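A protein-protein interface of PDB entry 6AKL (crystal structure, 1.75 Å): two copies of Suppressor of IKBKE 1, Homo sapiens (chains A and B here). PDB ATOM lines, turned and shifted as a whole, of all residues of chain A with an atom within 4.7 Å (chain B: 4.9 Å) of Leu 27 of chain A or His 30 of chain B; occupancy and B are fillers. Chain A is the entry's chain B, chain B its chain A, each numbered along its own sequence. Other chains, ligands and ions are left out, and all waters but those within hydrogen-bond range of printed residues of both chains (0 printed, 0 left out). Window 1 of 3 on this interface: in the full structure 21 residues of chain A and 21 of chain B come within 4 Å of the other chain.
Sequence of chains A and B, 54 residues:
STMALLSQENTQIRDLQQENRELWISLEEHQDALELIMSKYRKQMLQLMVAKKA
The side-chain amide oxygen (OE1) of Gln 31 of chain A sits at hydrogen-bond distance from a ring nitrogen (NE2) of His 30 of chain B (2.7 Å). The side-chain amide nitrogen (NE2) of Gln 31 of chain B is in hydrogen-bond range of a ring nitrogen (NE2) of His 30 of chain A, 3.3 Å away.
Leu 23 of chain B touches its own counterpart, Leu 23 of chain A. Leu 27 of chain A touches its own counterpart, Leu 27 of chain B. Leu 34 of chain A touches His 30 of chain B, but with the chains exchanged His 30 of chain A does not touch Leu 34 of chain B (4.2 Å). Leu 34 of chain A touches its own counterpart, Leu 34 of chain B. Positions printed for both chains: 23, 26, 27, 28, 29, 30, 31 and 34. Of the 14 pairs that touch across the chains among the printed residues, 12 have their exchanged pair printed and touching as well.
Of the printed residues of chain B, Trp 24 of chain A touches Leu 23. Printed residues of chain B within 4 Å of Leu 27 of chain A: Leu 23 (3.8 Å), Ser 26 (3.5 Å), Leu 27 (3.6 Å) and His 30 (3.6 Å). His 30 of chain B touches four residues of chain A. Of the printed residues of chain A, Leu 34 of chain B touches Leu 34 (3.8 Å).
Of the 10 printed residues of chain A, 7 touch a printed residue of chain B. Hydrophobic or aromatic side chains of chain A within 4 Å of the printed part of chain B: Leu 23, Trp 24, Leu 27, His 30 and Leu 34. Of the 10 printed residues of chain B, 6 touch a printed residue of chain A. Along chain B the printed residues that touch a printed residue of chain A span positions 23 to 34. Among the printed residues, 14 pairs touch across the chains. Among the printed residues, no Asp or Glu carboxylate lies within 4 Å of a Lys or Arg side-chain nitrogen of the other chain.
Among the printed residues, pairs that only touch across the chains: Leu 23 of chain A with Leu 23 of chain B, Leu 23 of chain A with Leu 27 of chain B, Trp 24 of chain A with Leu 23 of chain B, Ser 26 of chain A with Leu 27 of chain B, Leu 27 of chain A with Leu 23 of chain B, Leu 27 of chain A with Ser 26 of chain B, Leu 27 of chain A with Leu 27 of chain B, Leu 27 of chain A with His 30 of chain B, His 30 of chain A with Leu 27 of chain B, His 30 of chain A with His 30 of chain B, Leu 34 of chain A with His 30 of chain B and Leu 34 of chain A with Leu 34 of chain B.
The backbone carbonyl oxygen (O) of Ser 26 of chain B is in hydrogen-bond range of a ring nitrogen (ND1) of His 30 of chain B (2.8 Å). ND1 of His 30 of chain A lies within hydrogen-bond range of O of Ser 26 of chain A (2.8 Å).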
ATOM      1  N   LEU A  23      29.623  31.264   3.769  1.00  0.00           N
ATOM      2  CA  LEU A  23      29.640  29.887   3.280  1.00  0.00           C
ATOM      3  C   LEU A  23      28.399  29.574   2.457  1.00  0.00           C
ATOM      4  O   LEU A  23      28.483  28.864   1.436  1.00  0.00           O
ATOM      5  CB  LEU A  23      29.747  28.932   4.475  1.00  0.00           C
ATOM      6  CG  LEU A  23      31.128  28.910   5.130  1.00  0.00           C
ATOM      7  CD1 LEU A  23      31.072  28.149   6.473  1.00  0.00           C
ATOM      8  CD2 LEU A  23      32.137  28.250   4.206  1.00  0.00           C
ATOM      9  N   TRP A  24      27.225  30.060   2.884  1.00  0.00           N
ATOM     10  CA  TRP A  24      26.029  29.812   2.075  1.00  0.00           C
ATOM     11  C   TRP A  24      26.168  30.450   0.698  1.00  0.00           C
ATOM     12  O   TRP A  24      25.761  29.857  -0.307  1.00  0.00           O
ATOM     13  CB  TRP A  24      24.773  30.337   2.770  1.00  0.00           C
ATOM     14  CG  TRP A  24      24.216  29.444   3.806  1.00  0.00           C
ATOM     15  CD1 TRP A  24      24.241  29.643   5.163  1.00  0.00           C
ATOM     16  CD2 TRP A  24      23.521  28.201   3.599  1.00  0.00           C
ATOM     17  NE1 TRP A  24      23.615  28.610   5.801  1.00  0.00           N
ATOM     18  CE2 TRP A  24      23.160  27.712   4.872  1.00  0.00           C
ATOM     19  CE3 TRP A  24      23.169  27.467   2.467  1.00  0.00           C
ATOM     20  CZ2 TRP A  24      22.460  26.513   5.043  1.00  0.00           C
ATOM     21  CZ3 TRP A  24      22.477  26.253   2.636  1.00  0.00           C
ATOM     22  CH2 TRP A  24      22.127  25.799   3.918  1.00  0.00           C
ATOM     23  N   ILE A  25      26.763  31.642   0.631  1.00  0.00           N
ATOM     24  CA  ILE A  25      26.966  32.318  -0.657  1.00  0.00           C
ATOM     25  C   ILE A  25      27.909  31.514  -1.543  1.00  0.00           C
ATOM     26  O   ILE A  25      27.651  31.322  -2.740  1.00  0.00           O
ATOM     27  CB  ILE A  25      27.480  33.757  -0.436  1.00  0.00           C
ATOM     28  CG1 ILE A  25      26.341  34.644   0.055  1.00  0.00           C
ATOM     29  CG2 ILE A  25      28.062  34.343  -1.755  1.00  0.00           C
ATOM     30  CD1 ILE A  25      26.803  35.917   0.752  1.00  0.00           C
ATOM     31  N   SER A  26      29.016  31.037  -0.979  1.00  0.00           N
ATOM     32  CA  SER A  26      29.947  30.245  -1.779  1.00  0.00           C
ATOM     33  C   SER A  26      29.299  28.951  -2.262  1.00  0.00           C
ATOM     34  O   SER A  26      29.527  28.511  -3.398  1.00  0.00           O
ATOM     35  CB  SER A  26      31.208  29.927  -0.979  1.00  0.00           C
ATOM     36  OG  SER A  26      32.117  29.196  -1.792  1.00  0.00           O
ATOM     37  N   LEU A  27      28.490  28.326  -1.417  1.00  0.00           N
ATOM     38  CA  LEU A  27      27.866  27.070  -1.828  1.00  0.00           C
ATOM     39  C   LEU A  27      26.893  27.314  -2.976  1.00  0.00           C
ATOM     40  O   LEU A  27      26.822  26.509  -3.914  1.00  0.00           O
ATOM     41  CB  LEU A  27      27.169  26.422  -0.631  1.00  0.00           C
ATOM     42  CG  LEU A  27      26.562  25.039  -0.885  1.00  0.00           C
ATOM     43  CD1 LEU A  27      27.666  24.059  -1.333  1.00  0.00           C
ATOM     44  CD2 LEU A  27      25.880  24.541   0.388  1.00  0.00           C
ATOM     45  N   GLU A  28      26.182  28.447  -2.944  1.00  0.00           N
ATOM     46  CA  GLU A  28      25.302  28.806  -4.051  1.00  0.00           C
ATOM     47  C   GLU A  28      26.087  28.934  -5.344  1.00  0.00           C
ATOM     48  O   GLU A  28      25.651  28.447  -6.395  1.00  0.00           O
ATOM     49  CB  GLU A  28      24.567  30.125  -3.752  1.00  0.00           C
ATOM     50  CG  GLU A  28      23.490  30.471  -4.783  1.00  0.00           C
ATOM     51  CD  GLU A  28      22.902  31.879  -4.616  1.00  0.00           C
ATOM     52  OE1 GLU A  28      23.416  32.668  -3.790  1.00  0.00           O
ATOM     53  OE2 GLU A  28      21.928  32.200  -5.335  1.00  0.00           O
ATOM     54  N   GLU A  29      27.250  29.581  -5.281  1.00  0.00           N
ATOM     55  CA  GLU A  29      28.076  29.732  -6.477  1.00  0.00           C
ATOM     56  C   GLU A  29      28.584  28.378  -6.965  1.00  0.00           C
ATOM     57  O   GLU A  29      28.584  28.115  -8.172  1.00  0.00           O
ATOM     58  CB  GLU A  29      29.238  30.682  -6.181  1.00  0.00           C
ATOM     59  CG  GLU A  29      28.725  32.089  -5.886  1.00  0.00           C
ATOM     60  CD  GLU A  29      29.794  33.047  -5.412  1.00  0.00           C
ATOM     61  OE1 GLU A  29      30.952  32.619  -5.198  1.00  0.00           O
ATOM     62  OE2 GLU A  29      29.458  34.243  -5.244  1.00  0.00           O
ATOM     63  N   HIS A  30      29.017  27.503  -6.046  1.00  0.00           N
ATOM     64  CA  HIS A  30      29.476  26.171  -6.456  1.00  0.00           C
ATOM     65  C   HIS A  30      28.338  25.335  -7.034  1.00  0.00           C
ATOM     66  O   HIS A  30      28.534  24.597  -8.013  1.00  0.00           O
ATOM     67  CB  HIS A  30      30.125  25.431  -5.278  1.00  0.00           C
ATOM     68  CG  HIS A  30      31.517  25.886  -4.963  1.00  0.00           C
ATOM     69  ND1 HIS A  30      31.790  27.126  -4.425  1.00  0.00           N
ATOM     70  CD2 HIS A  30      32.717  25.281  -5.144  1.00  0.00           C
ATOM     71  CE1 HIS A  30      33.094  27.254  -4.260  1.00  0.00           C
ATOM     72  NE2 HIS A  30      33.681  26.149  -4.689  1.00  0.00           N
ATOM     73  N   GLN A  31      27.144  25.413  -6.444  1.00  0.00           N
ATOM     74  CA  GLN A  31      26.021  24.654  -6.993  1.00  0.00           C
ATOM     75  C   GLN A  31      25.648  25.161  -8.386  1.00  0.00           C
ATOM     76  O   GLN A  31      25.397  24.362  -9.286  1.00  0.00           O
ATOM     77  CB  GLN A  31      24.817  24.720  -6.046  1.00  0.00           C
ATOM     78  CG  GLN A  31      23.568  23.948  -6.555  1.00  0.00           C
ATOM     79  CD  GLN A  31      23.768  22.425  -6.742  1.00  0.00           C
ATOM     80  OE1 GLN A  31      24.532  21.768  -6.023  1.00  0.00           O
ATOM     81  NE2 GLN A  31      23.042  21.862  -7.702  1.00  0.00           N
ATOM     82  N   LEU A  34      28.265  23.995 -10.878  1.00  0.00           N
ATOM     83  CA  LEU A  34      28.144  22.576 -11.182  1.00  0.00           C
ATOM     84  C   LEU A  34      26.978  22.337 -12.130  1.00  0.00           C
ATOM     85  O   LEU A  34      27.090  21.553 -13.082  1.00  0.00           O
ATOM     86  CB  LEU A  34      27.980  21.771  -9.884  1.00  0.00           C
ATOM     87  CG  LEU A  34      27.844  20.250  -9.971  1.00  0.00           C
ATOM     88  CD1 LEU A  34      29.042  19.672 -10.716  1.00  0.00           C
ATOM     89  CD2 LEU A  34      27.733  19.639  -8.563  1.00  0.00           C
ATOM     90  N   LEU B  23      28.532  23.013   5.791  1.00  0.00           N
ATOM     91  CA  LEU B  23      28.693  23.816   4.576  1.00  0.00           C
ATOM     92  C   LEU B  23      30.081  23.621   3.979  1.00  0.00           C
ATOM     93  O   LEU B  23      30.227  23.476   2.752  1.00  0.00           O
ATOM     94  CB  LEU B  23      28.416  25.297   4.902  1.00  0.00           C
ATOM     95  CG  LEU B  23      26.963  25.636   5.291  1.00  0.00           C
ATOM     96  CD1 LEU B  23      26.863  27.061   5.871  1.00  0.00           C
ATOM     97  CD2 LEU B  23      26.040  25.521   4.084  1.00  0.00           C
ATOM     98  N   SER B  26      30.133  20.288   2.274  1.00  0.00           N
ATOM     99  CA  SER B  26      29.424  20.330   0.994  1.00  0.00           C
ATOM    100  C   SER B  26      30.236  21.069  -0.061  1.00  0.00           C
ATOM    101  O   SER B  26      30.233  20.681  -1.235  1.00  0.00           O
ATOM    102  CB  SER B  26      28.048  20.979   1.156  1.00  0.00           C
ATOM    103  OG  SER B  26      27.271  20.813  -0.031  1.00  0.00           O
ATOM    104  N   LEU B  27      30.945  22.130   0.330  1.00  0.00           N
ATOM    105  CA  LEU B  27      31.812  22.815  -0.632  1.00  0.00           C
ATOM    106  C   LEU B  27      32.891  21.881  -1.168  1.00  0.00           C
ATOM    107  O   LEU B  27      33.167  21.859  -2.382  1.00  0.00           O
ATOM    108  CB  LEU B  27      32.450  24.043   0.021  1.00  0.00           C
ATOM    109  CG  LEU B  27      31.451  25.187   0.171  1.00  0.00           C
ATOM    110  CD1 LEU B  27      31.980  26.210   1.192  1.00  0.00           C
ATOM    111  CD2 LEU B  27      31.240  25.894  -1.164  1.00  0.00           C
ATOM    112  N   GLU B  28      33.546  21.133  -0.273  1.00  0.00           N
ATOM    113  CA  GLU B  28      34.555  20.168  -0.707  1.00  0.00           C
ATOM    114  C   GLU B  28      33.948  19.118  -1.623  1.00  0.00           C
ATOM    115  O   GLU B  28      34.556  18.729  -2.626  1.00  0.00           O
ATOM    116  CB  GLU B  28      35.198  19.482   0.500  1.00  0.00           C
ATOM    117  CG  GLU B  28      35.989  20.398   1.412  1.00  0.00           C
ATOM    118  CD  GLU B  28      36.582  19.645   2.592  1.00  0.00           C
ATOM    119  OE1 GLU B  28      35.955  19.631   3.674  1.00  0.00           O
ATOM    120  OE2 GLU B  28      37.672  19.056   2.430  1.00  0.00           O
ATOM    121  N   GLU B  29      32.740  18.656  -1.300  1.00  0.00           N
ATOM    122  CA  GLU B  29      32.063  17.684  -2.152  1.00  0.00           C
ATOM    123  C   GLU B  29      31.762  18.258  -3.533  1.00  0.00           C
ATOM    124  O   GLU B  29      31.918  17.565  -4.548  1.00  0.00           O
ATOM    125  CB  GLU B  29      30.778  17.185  -1.461  1.00  0.00           C
ATOM    126  CG  GLU B  29      31.082  16.271  -0.259  1.00  0.00           C
ATOM    127  CD  GLU B  29      29.876  15.968   0.653  1.00  0.00           C
ATOM    128  OE1 GLU B  29      28.857  16.700   0.613  1.00  0.00           O
ATOM    129  OE2 GLU B  29      29.978  14.997   1.442  1.00  0.00           O
ATOM    130  N   HIS B  30      31.337  19.519  -3.593  1.00  0.00           N
ATOM    131  CA  HIS B  30      31.113  20.179  -4.876  1.00  0.00           C
ATOM    132  C   HIS B  30      32.407  20.312  -5.680  1.00  0.00           C
ATOM    133  O   HIS B  30      32.409  20.083  -6.890  1.00  0.00           O
ATOM    134  CB  HIS B  30      30.489  21.558  -4.654  1.00  0.00           C
ATOM    135  CG  HIS B  30      29.008  21.515  -4.480  1.00  0.00           C
ATOM    136  ND1 HIS B  30      28.413  21.088  -3.312  1.00  0.00           N
ATOM    137  CD2 HIS B  30      28.001  21.790  -5.343  1.00  0.00           C
ATOM    138  CE1 HIS B  30      27.099  21.138  -3.449  1.00  0.00           C
ATOM    139  NE2 HIS B  30      26.822  21.569  -4.666  1.00  0.00           N
ATOM    140  N   GLN B  31      33.517  20.708  -5.039  1.00  0.00           N
ATOM    141  CA  GLN B  31      34.784  20.796  -5.778  1.00  0.00           C
ATOM    142  C   GLN B  31      35.251  19.422  -6.256  1.00  0.00           C
ATOM    143  O   GLN B  31      35.753  19.291  -7.378  1.00  0.00           O
ATOM    144  CB  GLN B  31      35.847  21.482  -4.908  1.00  0.00           C
ATOM    145  CG  GLN B  31      35.530  22.960  -4.672  1.00  0.00           C
ATOM    146  CD  GLN B  31      36.637  23.725  -3.943  1.00  0.00           C
ATOM    147  OE1 GLN B  31      37.825  23.410  -4.071  1.00  0.00           O
ATOM    148  NE2 GLN B  31      36.241  24.734  -3.166  1.00  0.00           N
ATOM    149  N   ASP B  32      35.082  18.373  -5.438  1.00  0.00           N
ATOM    150  CA  ASP B  32      35.434  17.027  -5.895  1.00  0.00           C
ATOM    151  C   ASP B  32      34.610  16.634  -7.116  1.00  0.00           C
ATOM    152  O   ASP B  32      35.140  16.102  -8.106  1.00  0.00           O
ATOM    153  CB  ASP B  32      35.213  16.013  -4.769  1.00  0.00           C
ATOM    154  CG  ASP B  32      36.221  16.153  -3.631  1.00  0.00           C
ATOM    155  OD1 ASP B  32      37.192  16.932  -3.758  1.00  0.00           O
ATOM    156  OD2 ASP B  32      36.023  15.488  -2.591  1.00  0.00           O
ATOM    157  N   ALA B  33      33.298  16.876  -7.056  1.00  0.00           N
ATOM    158  CA  ALA B  33      32.423  16.571  -8.185  1.00  0.00           C
ATOM    159  C   ALA B  33      32.798  17.373  -9.428  1.00  0.00           C
ATOM    160  O   ALA B  33      32.773  16.844 -10.547  1.00  0.00           O
ATOM    161  CB  ALA B  33      30.963  16.845  -7.800  1.00  0.00           C
ATOM    162  N   LEU B  34      33.114  18.657  -9.262  1.00  0.00           N
ATOM    163  CA  LEU B  34      33.476  19.494 -10.404  1.00  0.00           C
ATOM    164  C   LEU B  34      34.753  19.008 -11.080  1.00  0.00           C
ATOM    165  O   LEU B  34      34.839  18.973 -12.313  1.00  0.00           O
ATOM    166  CB  LEU B  34      33.655  20.941  -9.949  1.00  0.00           C
ATOM    167  CG  LEU B  34      32.411  21.782  -9.657  1.00  0.00           C
ATOM    168  CD1 LEU B  34      32.722  22.829  -8.601  1.00  0.00           C
ATOM    169  CD2 LEU B  34      31.948  22.426 -10.926  1.00  0.00           C
